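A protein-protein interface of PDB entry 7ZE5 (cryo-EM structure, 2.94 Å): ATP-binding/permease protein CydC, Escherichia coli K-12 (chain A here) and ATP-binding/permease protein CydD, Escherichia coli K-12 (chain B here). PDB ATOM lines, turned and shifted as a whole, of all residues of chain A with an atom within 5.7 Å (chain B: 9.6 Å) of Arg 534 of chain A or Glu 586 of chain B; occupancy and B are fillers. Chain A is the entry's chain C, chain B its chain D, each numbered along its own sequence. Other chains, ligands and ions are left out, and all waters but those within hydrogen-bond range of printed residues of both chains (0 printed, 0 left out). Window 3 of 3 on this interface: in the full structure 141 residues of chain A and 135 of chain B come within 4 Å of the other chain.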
ATOM      1  N   ALA A 507      19.201  19.141 -19.886  1.00  0.00           N
ATOM      2  CA  ALA A 507      19.911  17.880 -20.070  1.00  0.00           C
ATOM      3  C   ALA A 507      20.858  17.941 -21.260  1.00  0.00           C
ATOM      4  O   ALA A 507      21.934  17.334 -21.236  1.00  0.00           O
ATOM      5  CB  ALA A 507      18.911  16.739 -20.237  1.00  0.00           C
ATOM      6  N   THR A 508      20.475  18.660 -22.317  1.00  0.00           N
ATOM      7  CA  THR A 508      21.332  18.742 -23.496  1.00  0.00           C
ATOM      8  C   THR A 508      22.572  19.584 -23.228  1.00  0.00           C
ATOM      9  O   THR A 508      23.681  19.207 -23.624  1.00  0.00           O
ATOM     10  CB  THR A 508      20.552  19.306 -24.681  1.00  0.00           C
ATOM     11  OG1 THR A 508      19.356  18.543 -24.875  1.00  0.00           O
ATOM     12  CG2 THR A 508      21.390  19.245 -25.942  1.00  0.00           C
ATOM     13  N   GLU A 510      23.829  20.314 -20.177  1.00  0.00           N
ATOM     14  CA  GLU A 510      24.609  19.653 -19.138  1.00  0.00           C
ATOM     15  C   GLU A 510      25.423  18.503 -19.713  1.00  0.00           C
ATOM     16  O   GLU A 510      26.576  18.295 -19.324  1.00  0.00           O
ATOM     17  CB  GLU A 510      23.689  19.161 -18.023  1.00  0.00           C
ATOM     18  CG  GLU A 510      24.394  18.389 -16.930  1.00  0.00           C
ATOM     19  CD  GLU A 510      23.460  17.465 -16.177  1.00  0.00           C
ATOM     20  OE1 GLU A 510      22.300  17.311 -16.611  1.00  0.00           O
ATOM     21  OE2 GLU A 510      23.886  16.893 -15.151  1.00  0.00           O
ATOM     22  N   SER A 511      24.839  17.745 -20.644  1.00  0.00           N
ATOM     23  CA  SER A 511      25.593  16.689 -21.311  1.00  0.00           C
ATOM     24  C   SER A 511      26.771  17.262 -22.083  1.00  0.00           C
ATOM     25  O   SER A 511      27.877  16.713 -22.042  1.00  0.00           O
ATOM     26  CB  SER A 511      24.682  15.906 -22.252  1.00  0.00           C
ATOM     27  OG  SER A 511      23.752  15.123 -21.532  1.00  0.00           O
ATOM     28  N   LEU A 514      29.373  18.633 -19.414  1.00  0.00           N
ATOM     29  CA  LEU A 514      30.087  17.547 -18.751  1.00  0.00           C
ATOM     30  C   LEU A 514      31.024  16.834 -19.716  1.00  0.00           C
ATOM     31  O   LEU A 514      32.101  16.375 -19.323  1.00  0.00           O
ATOM     32  CB  LEU A 514      29.093  16.563 -18.137  1.00  0.00           C
ATOM     33  CG  LEU A 514      28.337  17.057 -16.905  1.00  0.00           C
ATOM     34  CD1 LEU A 514      27.295  16.045 -16.482  1.00  0.00           C
ATOM     35  CD2 LEU A 514      29.302  17.335 -15.768  1.00  0.00           C
ATOM     36  N   MET A 528      34.982  18.392  -7.827  1.00  0.00           N
ATOM     37  CA  MET A 528      33.666  18.743  -8.419  1.00  0.00           C
ATOM     38  C   MET A 528      32.533  18.524  -7.414  1.00  0.00           C
ATOM     39  O   MET A 528      32.240  17.357  -7.085  1.00  0.00           O
ATOM     40  CB  MET A 528      33.393  17.915  -9.679  1.00  0.00           C
ATOM     41  CG  MET A 528      32.066  18.238 -10.341  1.00  0.00           C
ATOM     42  SD  MET A 528      31.785  17.265 -11.842  1.00  0.00           S
ATOM     43  CE  MET A 528      30.175  17.879 -12.336  1.00  0.00           C
ATOM     44  N   ARG A 532      23.954  16.955  -8.300  1.00  0.00           N
ATOM     45  CA  ARG A 532      23.552  16.108  -9.456  1.00  0.00           C
ATOM     46  C   ARG A 532      24.456  14.872  -9.505  1.00  0.00           C
ATOM     47  O   ARG A 532      25.684  15.046  -9.589  1.00  0.00           O
ATOM     48  CB  ARG A 532      23.655  16.915 -10.754  1.00  0.00           C
ATOM     49  CG  ARG A 532      22.959  18.268 -10.701  1.00  0.00           C
ATOM     50  CD  ARG A 532      21.500  18.220 -11.116  1.00  0.00           C
ATOM     51  NE  ARG A 532      21.334  18.344 -12.558  1.00  0.00           N
ATOM     52  CZ  ARG A 532      21.068  19.482 -13.190  1.00  0.00           C
ATOM     53  NH1 ARG A 532      20.936  19.495 -14.506  1.00  0.00           N
ATOM     54  NH2 ARG A 532      20.931  20.603 -12.506  1.00  0.00           N
ATOM     55  N   LEU A 533      23.860  13.676  -9.480  1.00  0.00           N
ATOM     56  CA  LEU A 533      24.614  12.434  -9.479  1.00  0.00           C
ATOM     57  C   LEU A 533      24.888  11.906 -10.882  1.00  0.00           C
ATOM     58  O   LEU A 533      25.125  10.704 -11.040  1.00  0.00           O
ATOM     59  CB  LEU A 533      23.877  11.381  -8.658  1.00  0.00           C
ATOM     60  CG  LEU A 533      23.227  11.955  -7.402  1.00  0.00           C
ATOM     61  CD1 LEU A 533      22.330  10.918  -6.796  1.00  0.00           C
ATOM     62  CD2 LEU A 533      24.275  12.411  -6.398  1.00  0.00           C
ATOM     63  N   ARG A 534      24.856  12.765 -11.897  1.00  0.00           N
ATOM     64  CA  ARG A 534      25.104  12.316 -13.259  1.00  0.00           C
ATOM     65  C   ARG A 534      26.593  12.343 -13.570  1.00  0.00           C
ATOM     66  O   ARG A 534      27.310  13.268 -13.180  1.00  0.00           O
ATOM     67  CB  ARG A 534      24.350  13.187 -14.260  1.00  0.00           C
ATOM     68  CG  ARG A 534      24.490  12.720 -15.692  1.00  0.00           C
ATOM     69  CD  ARG A 534      23.660  13.563 -16.622  1.00  0.00           C
ATOM     70  NE  ARG A 534      23.819  13.137 -18.006  1.00  0.00           N
ATOM     71  CZ  ARG A 534      23.188  13.700 -19.028  1.00  0.00           C
ATOM     72  NH1 ARG A 534      23.384  13.253 -20.261  1.00  0.00           N
ATOM     73  NH2 ARG A 534      22.362  14.714 -18.817  1.00  0.00           N
ATOM     74  N   GLY A 535      27.054  11.320 -14.280  1.00  0.00           N
ATOM     75  CA  GLY A 535      28.447  11.240 -14.675  1.00  0.00           C
ATOM     76  C   GLY A 535      29.411  11.069 -13.523  1.00  0.00           C
ATOM     77  O   GLY A 535      30.538  11.579 -13.582  1.00  0.00           O
ATOM     78  N   LEU A 536      29.003  10.357 -12.477  1.00  0.00           N
ATOM     79  CA  LEU A 536      29.858  10.105 -11.326  1.00  0.00           C
ATOM     80  C   LEU A 536      30.634   8.801 -11.444  1.00  0.00           C
ATOM     81  O   LEU A 536      31.452   8.502 -10.568  1.00  0.00           O
ATOM     82  CB  LEU A 536      29.022  10.090 -10.045  1.00  0.00           C
ATOM     83  CG  LEU A 536      28.420  11.428  -9.617  1.00  0.00           C
ATOM     84  CD1 LEU A 536      27.917  11.352  -8.188  1.00  0.00           C
ATOM     85  CD2 LEU A 536      29.435  12.541  -9.771  1.00  0.00           C
ATOM     86  N   HIS B 542      14.223  21.851 -15.003  1.00  0.00           N
ATOM     87  CA  HIS B 542      15.049  20.962 -15.806  1.00  0.00           C
ATOM     88  C   HIS B 542      14.817  19.493 -15.485  1.00  0.00           C
ATOM     89  O   HIS B 542      15.168  18.636 -16.303  1.00  0.00           O
ATOM     90  CB  HIS B 542      16.533  21.297 -15.619  1.00  0.00           C
ATOM     91  CG  HIS B 542      16.984  21.268 -14.193  1.00  0.00           C
ATOM     92  ND1 HIS B 542      16.719  22.286 -13.305  1.00  0.00           N
ATOM     93  CD2 HIS B 542      17.704  20.351 -13.507  1.00  0.00           C
ATOM     94  CE1 HIS B 542      17.244  21.990 -12.129  1.00  0.00           C
ATOM     95  NE2 HIS B 542      17.841  20.816 -12.223  1.00  0.00           N
ATOM     96  N   LEU B 544      12.775  16.302 -15.643  1.00  0.00           N
ATOM     97  CA  LEU B 544      11.749  15.836 -16.561  1.00  0.00           C
ATOM     98  C   LEU B 544      11.057  14.561 -16.106  1.00  0.00           C
ATOM     99  O   LEU B 544       9.940  14.295 -16.549  1.00  0.00           O
ATOM    100  CB  LEU B 544      12.341  15.611 -17.960  1.00  0.00           C
ATOM    101  CG  LEU B 544      13.105  16.787 -18.570  1.00  0.00           C
ATOM    102  CD1 LEU B 544      13.491  16.490 -20.006  1.00  0.00           C
ATOM    103  CD2 LEU B 544      12.283  18.060 -18.492  1.00  0.00           C
ATOM    104  N   ALA B 578      11.692  14.494 -26.424  1.00  0.00           N
ATOM    105  CA  ALA B 578      12.295  13.172 -26.296  1.00  0.00           C
ATOM    106  C   ALA B 578      13.812  13.248 -26.392  1.00  0.00           C
ATOM    107  O   ALA B 578      14.523  12.590 -25.625  1.00  0.00           O
ATOM    108  CB  ALA B 578      11.734  12.232 -27.362  1.00  0.00           C
ATOM    109  N   THR B 579      14.328  14.046 -27.330  1.00  0.00           N
ATOM    110  CA  THR B 579      15.774  14.220 -27.439  1.00  0.00           C
ATOM    111  C   THR B 579      16.336  14.910 -26.204  1.00  0.00           C
ATOM    112  O   THR B 579      17.423  14.564 -25.729  1.00  0.00           O
ATOM    113  CB  THR B 579      16.120  15.014 -28.696  1.00  0.00           C
ATOM    114  OG1 THR B 579      15.592  16.341 -28.583  1.00  0.00           O
ATOM    115  CG2 THR B 579      15.532  14.343 -29.927  1.00  0.00           C
ATOM    116  N   LEU B 580      15.610  15.895 -25.673  1.00  0.00           N
ATOM    117  CA  LEU B 580      16.048  16.554 -24.448  1.00  0.00           C
ATOM    118  C   LEU B 580      15.829  15.658 -23.234  1.00  0.00           C
ATOM    119  O   LEU B 580      16.514  15.812 -22.219  1.00  0.00           O
ATOM    120  CB  LEU B 580      15.320  17.889 -24.292  1.00  0.00           C
ATOM    121  CG  LEU B 580      15.589  18.777 -23.081  1.00  0.00           C
ATOM    122  CD1 LEU B 580      16.856  19.585 -23.273  1.00  0.00           C
ATOM    123  CD2 LEU B 580      14.421  19.700 -22.893  1.00  0.00           C
ATOM    124  N   LEU B 581      14.882  14.721 -23.321  1.00  0.00           N
ATOM    125  CA  LEU B 581      14.740  13.684 -22.306  1.00  0.00           C
ATOM    126  C   LEU B 581      15.687  12.514 -22.543  1.00  0.00           C
ATOM    127  O   LEU B 581      15.926  11.731 -21.617  1.00  0.00           O
ATOM    128  CB  LEU B 581      13.292  13.183 -22.270  1.00  0.00           C
ATOM    129  CG  LEU B 581      12.834  12.230 -21.166  1.00  0.00           C
ATOM    130  CD1 LEU B 581      13.383  12.651 -19.819  1.00  0.00           C
ATOM    131  CD2 LEU B 581      11.317  12.162 -21.125  1.00  0.00           C
ATOM    132  N   ALA B 582      16.233  12.384 -23.754  1.00  0.00           N
ATOM    133  CA  ALA B 582      17.172  11.303 -24.034  1.00  0.00           C
ATOM    134  C   ALA B 582      18.442  11.449 -23.207  1.00  0.00           C
ATOM    135  O   ALA B 582      18.968  10.460 -22.683  1.00  0.00           O
ATOM    136  CB  ALA B 582      17.506  11.267 -25.525  1.00  0.00           C
ATOM    137  N   HIS B 583      18.952  12.674 -23.083  1.00  0.00           N
ATOM    138  CA  HIS B 583      20.137  12.896 -22.265  1.00  0.00           C
ATOM    139  C   HIS B 583      19.846  12.667 -20.789  1.00  0.00           C
ATOM    140  O   HIS B 583      20.728  12.222 -20.047  1.00  0.00           O
ATOM    141  CB  HIS B 583      20.675  14.305 -22.501  1.00  0.00           C
ATOM    142  CG  HIS B 583      20.974  14.599 -23.937  1.00  0.00           C
ATOM    143  ND1 HIS B 583      19.987  14.826 -24.871  1.00  0.00           N
ATOM    144  CD2 HIS B 583      22.149  14.694 -24.602  1.00  0.00           C
ATOM    145  CE1 HIS B 583      20.541  15.052 -26.049  1.00  0.00           C
ATOM    146  NE2 HIS B 583      21.853  14.979 -25.912  1.00  0.00           N
ATOM    147  N   ARG B 584      18.627  12.964 -20.345  1.00  0.00           N
ATOM    148  CA  ARG B 584      18.189  12.523 -19.030  1.00  0.00           C
ATOM    149  C   ARG B 584      18.163  11.001 -18.982  1.00  0.00           C
ATOM    150  O   ARG B 584      17.870  10.334 -19.977  1.00  0.00           O
ATOM    151  CB  ARG B 584      16.804  13.082 -18.708  1.00  0.00           C
ATOM    152  CG  ARG B 584      16.796  14.510 -18.202  1.00  0.00           C
ATOM    153  CD  ARG B 584      16.909  14.544 -16.691  1.00  0.00           C
ATOM    154  NE  ARG B 584      17.519  15.781 -16.217  1.00  0.00           N
ATOM    155  CZ  ARG B 584      17.416  16.232 -14.972  1.00  0.00           C
ATOM    156  NH1 ARG B 584      18.007  17.368 -14.627  1.00  0.00           N
ATOM    157  NH2 ARG B 584      16.724  15.548 -14.072  1.00  0.00           N
ATOM    158  N   GLN B 585      18.492  10.458 -17.806  1.00  0.00           N
ATOM    159  CA  GLN B 585      18.625   9.023 -17.552  1.00  0.00           C
ATOM    160  C   GLN B 585      19.324   8.310 -18.705  1.00  0.00           C
ATOM    161  O   GLN B 585      18.965   7.182 -19.059  1.00  0.00           O
ATOM    162  CB  GLN B 585      17.263   8.374 -17.251  1.00  0.00           C
ATOM    163  CG  GLN B 585      16.193   8.460 -18.334  1.00  0.00           C
ATOM    164  CD  GLN B 585      14.803   8.169 -17.806  1.00  0.00           C
ATOM    165  OE1 GLN B 585      14.119   9.058 -17.300  1.00  0.00           O
ATOM    166  NE2 GLN B 585      14.377   6.916 -17.922  1.00  0.00           N
ATOM    167  N   GLU B 586      20.328   8.964 -19.295  1.00  0.00           N
ATOM    168  CA  GLU B 586      21.067   8.355 -20.395  1.00  0.00           C
ATOM    169  C   GLU B 586      21.896   7.172 -19.913  1.00  0.00           C
ATOM    170  O   GLU B 586      21.951   6.130 -20.578  1.00  0.00           O
ATOM    171  CB  GLU B 586      21.957   9.401 -21.065  1.00  0.00           C
ATOM    172  CG  GLU B 586      22.486   8.994 -22.426  1.00  0.00           C
ATOM    173  CD  GLU B 586      23.300  10.089 -23.080  1.00  0.00           C
ATOM    174  OE1 GLU B 586      23.593  11.098 -22.404  1.00  0.00           O
ATOM    175  OE2 GLU B 586      23.643   9.946 -24.273  1.00  0.00           O
ATOM    176  N   GLU B 587      22.544   7.311 -18.760  1.00  0.00           N
ATOM    177  CA  GLU B 587      23.347   6.246 -18.179  1.00  0.00           C
ATOM    178  C   GLU B 587      22.552   5.352 -17.238  1.00  0.00           C
ATOM    179  O   GLU B 587      23.118   4.410 -16.674  1.00  0.00           O
ATOM    180  CB  GLU B 587      24.549   6.840 -17.438  1.00  0.00           C
ATOM    181  CG  GLU B 587      25.546   7.537 -18.348  1.00  0.00           C
ATOM    182  CD  GLU B 587      26.612   8.290 -17.580  1.00  0.00           C
ATOM    183  OE1 GLU B 587      26.256   9.040 -16.646  1.00  0.00           O
ATOM    184  OE2 GLU B 587      27.807   8.131 -17.907  1.00  0.00           O
ATOM    185  N   ILE B 588      21.263   5.623 -17.054  1.00  0.00           N
ATOM    186  CA  ILE B 588      20.414   4.790 -16.213  1.00  0.00           C
ATOM    187  C   ILE B 588      19.255   4.233 -17.031  1.00  0.00           C
ATOM    188  O   ILE B 588      19.208   4.400 -18.250  1.00  0.00           O
ATOM    189  CB  ILE B 588      19.894   5.570 -14.995  1.00  0.00           C
ATOM    190  CG1 ILE B 588      21.023   5.803 -13.989  1.00  0.00           C
ATOM    191  CG2 ILE B 588      18.735   4.829 -14.345  1.00  0.00           C
ATOM    192  CD1 ILE B 588      20.555   6.366 -12.663  1.00  0.00           C
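A ring nitrogen (NE2) of His 542 of chain B sits at hydrogen-bond distance from the guanidinium group of Arg 532 of chain A, at 3.1 Å. NH1 of Arg 534 of chain A lies within hydrogen-bond range of O of His 583 of chain B (2.9 Å). NH1 of Arg 534 of chain A lies within salt-bridge range of OE1 of Glu 586 of chain B. The backbone NH (N) of Gly 535 of chain A lies within hydrogen-bond range of the side-chain carboxylate (OE1) of Glu 587 of chain B, at 3.4 Å.
The backbone carbonyl oxygen (O) of Ala 507 of chain A is in hydrogen-bond range of the side-chain hydroxyl (OG) of Ser 511 of chain A. The side-chain carboxylate (OE1) of Glu 510 of chain A lies within salt-bridge range of the guanidinium group (NH1) of Arg 532 of chain A, 3.3 Å away. The guanidinium group (NH2) of Arg 534 of chain A is in salt-bridge range of the side-chain carboxylate (OE1) of Glu 510 of chain A (3.4 Å). NH2 of Arg 534 of chain A sits close to OG of Ser 511 of chain A, 3.1 Å away. The backbone carbonyl oxygen (O) of Thr 579 of chain B sits at hydrogen-bond distance from a ring nitrogen (ND1) of His 583 of chain B (2.7 Å).
Leu 580 of chain B touches Ala 507 of chain A (O to CB, 3.2 Å). Ala 507 of chain A touches His 583 of chain B (O to CB, 3.5 Å). Arg 584 of chain B touches Ala 507 of chain A (CG to CB, 3.7 Å). Thr 508 of chain A touches Leu 580 of chain B (OG1 to CD1, 3.1 Å). Thr 508 of chain A touches His 583 of chain B (OG1 to ND1, 3.8 Å). His 583 of chain B touches Ser 511 of chain A (CB to OG, 3.3 Å). NH1 of Arg 584 of chain B touches NH1 of Arg 532 of chain A, 3.6 Å away.
Ala 507 of chain A touches just these residues of chain B: Leu 580, His 583 and Arg 584. Of the printed residues of chain B, Thr 508 of chain A touches Leu 580 and His 583. Printed residues of chain B within 4 Å of Ser 511 of chain A: His 583. Arg 534 of chain A touches two residues of chain B. Leu 536 of chain A touches none of the printed residues of chain B. Of the printed residues of chain A, His 542 of chain B touches Arg 532 (3.1 Å). Leu 544 of chain B touches none of the printed residues of chain A. Printed residues of chain A within 4 Å of Arg 584 of chain B: Ala 507 (3.7 Å) and Arg 532 (3.6 Å). Glu 586 of chain B touches just one residue of chain A: Arg 534. The nearest printed residue of chain B that does not touch Arg 532 of chain A is Leu 544 of chain B (8.8 Å).
Printed residues of chain B that touch a printed residue of chain A: His 542, Leu 580, His 583, Arg 584, Glu 586 and Glu 587. Along chain B the printed residues that touch a printed residue of chain A span positions 542 to 587. Among the printed residues, Asp or Glu carboxylates within 4 Å of a Lys or Arg side-chain nitrogen of the other chain: Arg 534 of chain A with Glu 586 of chain B.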
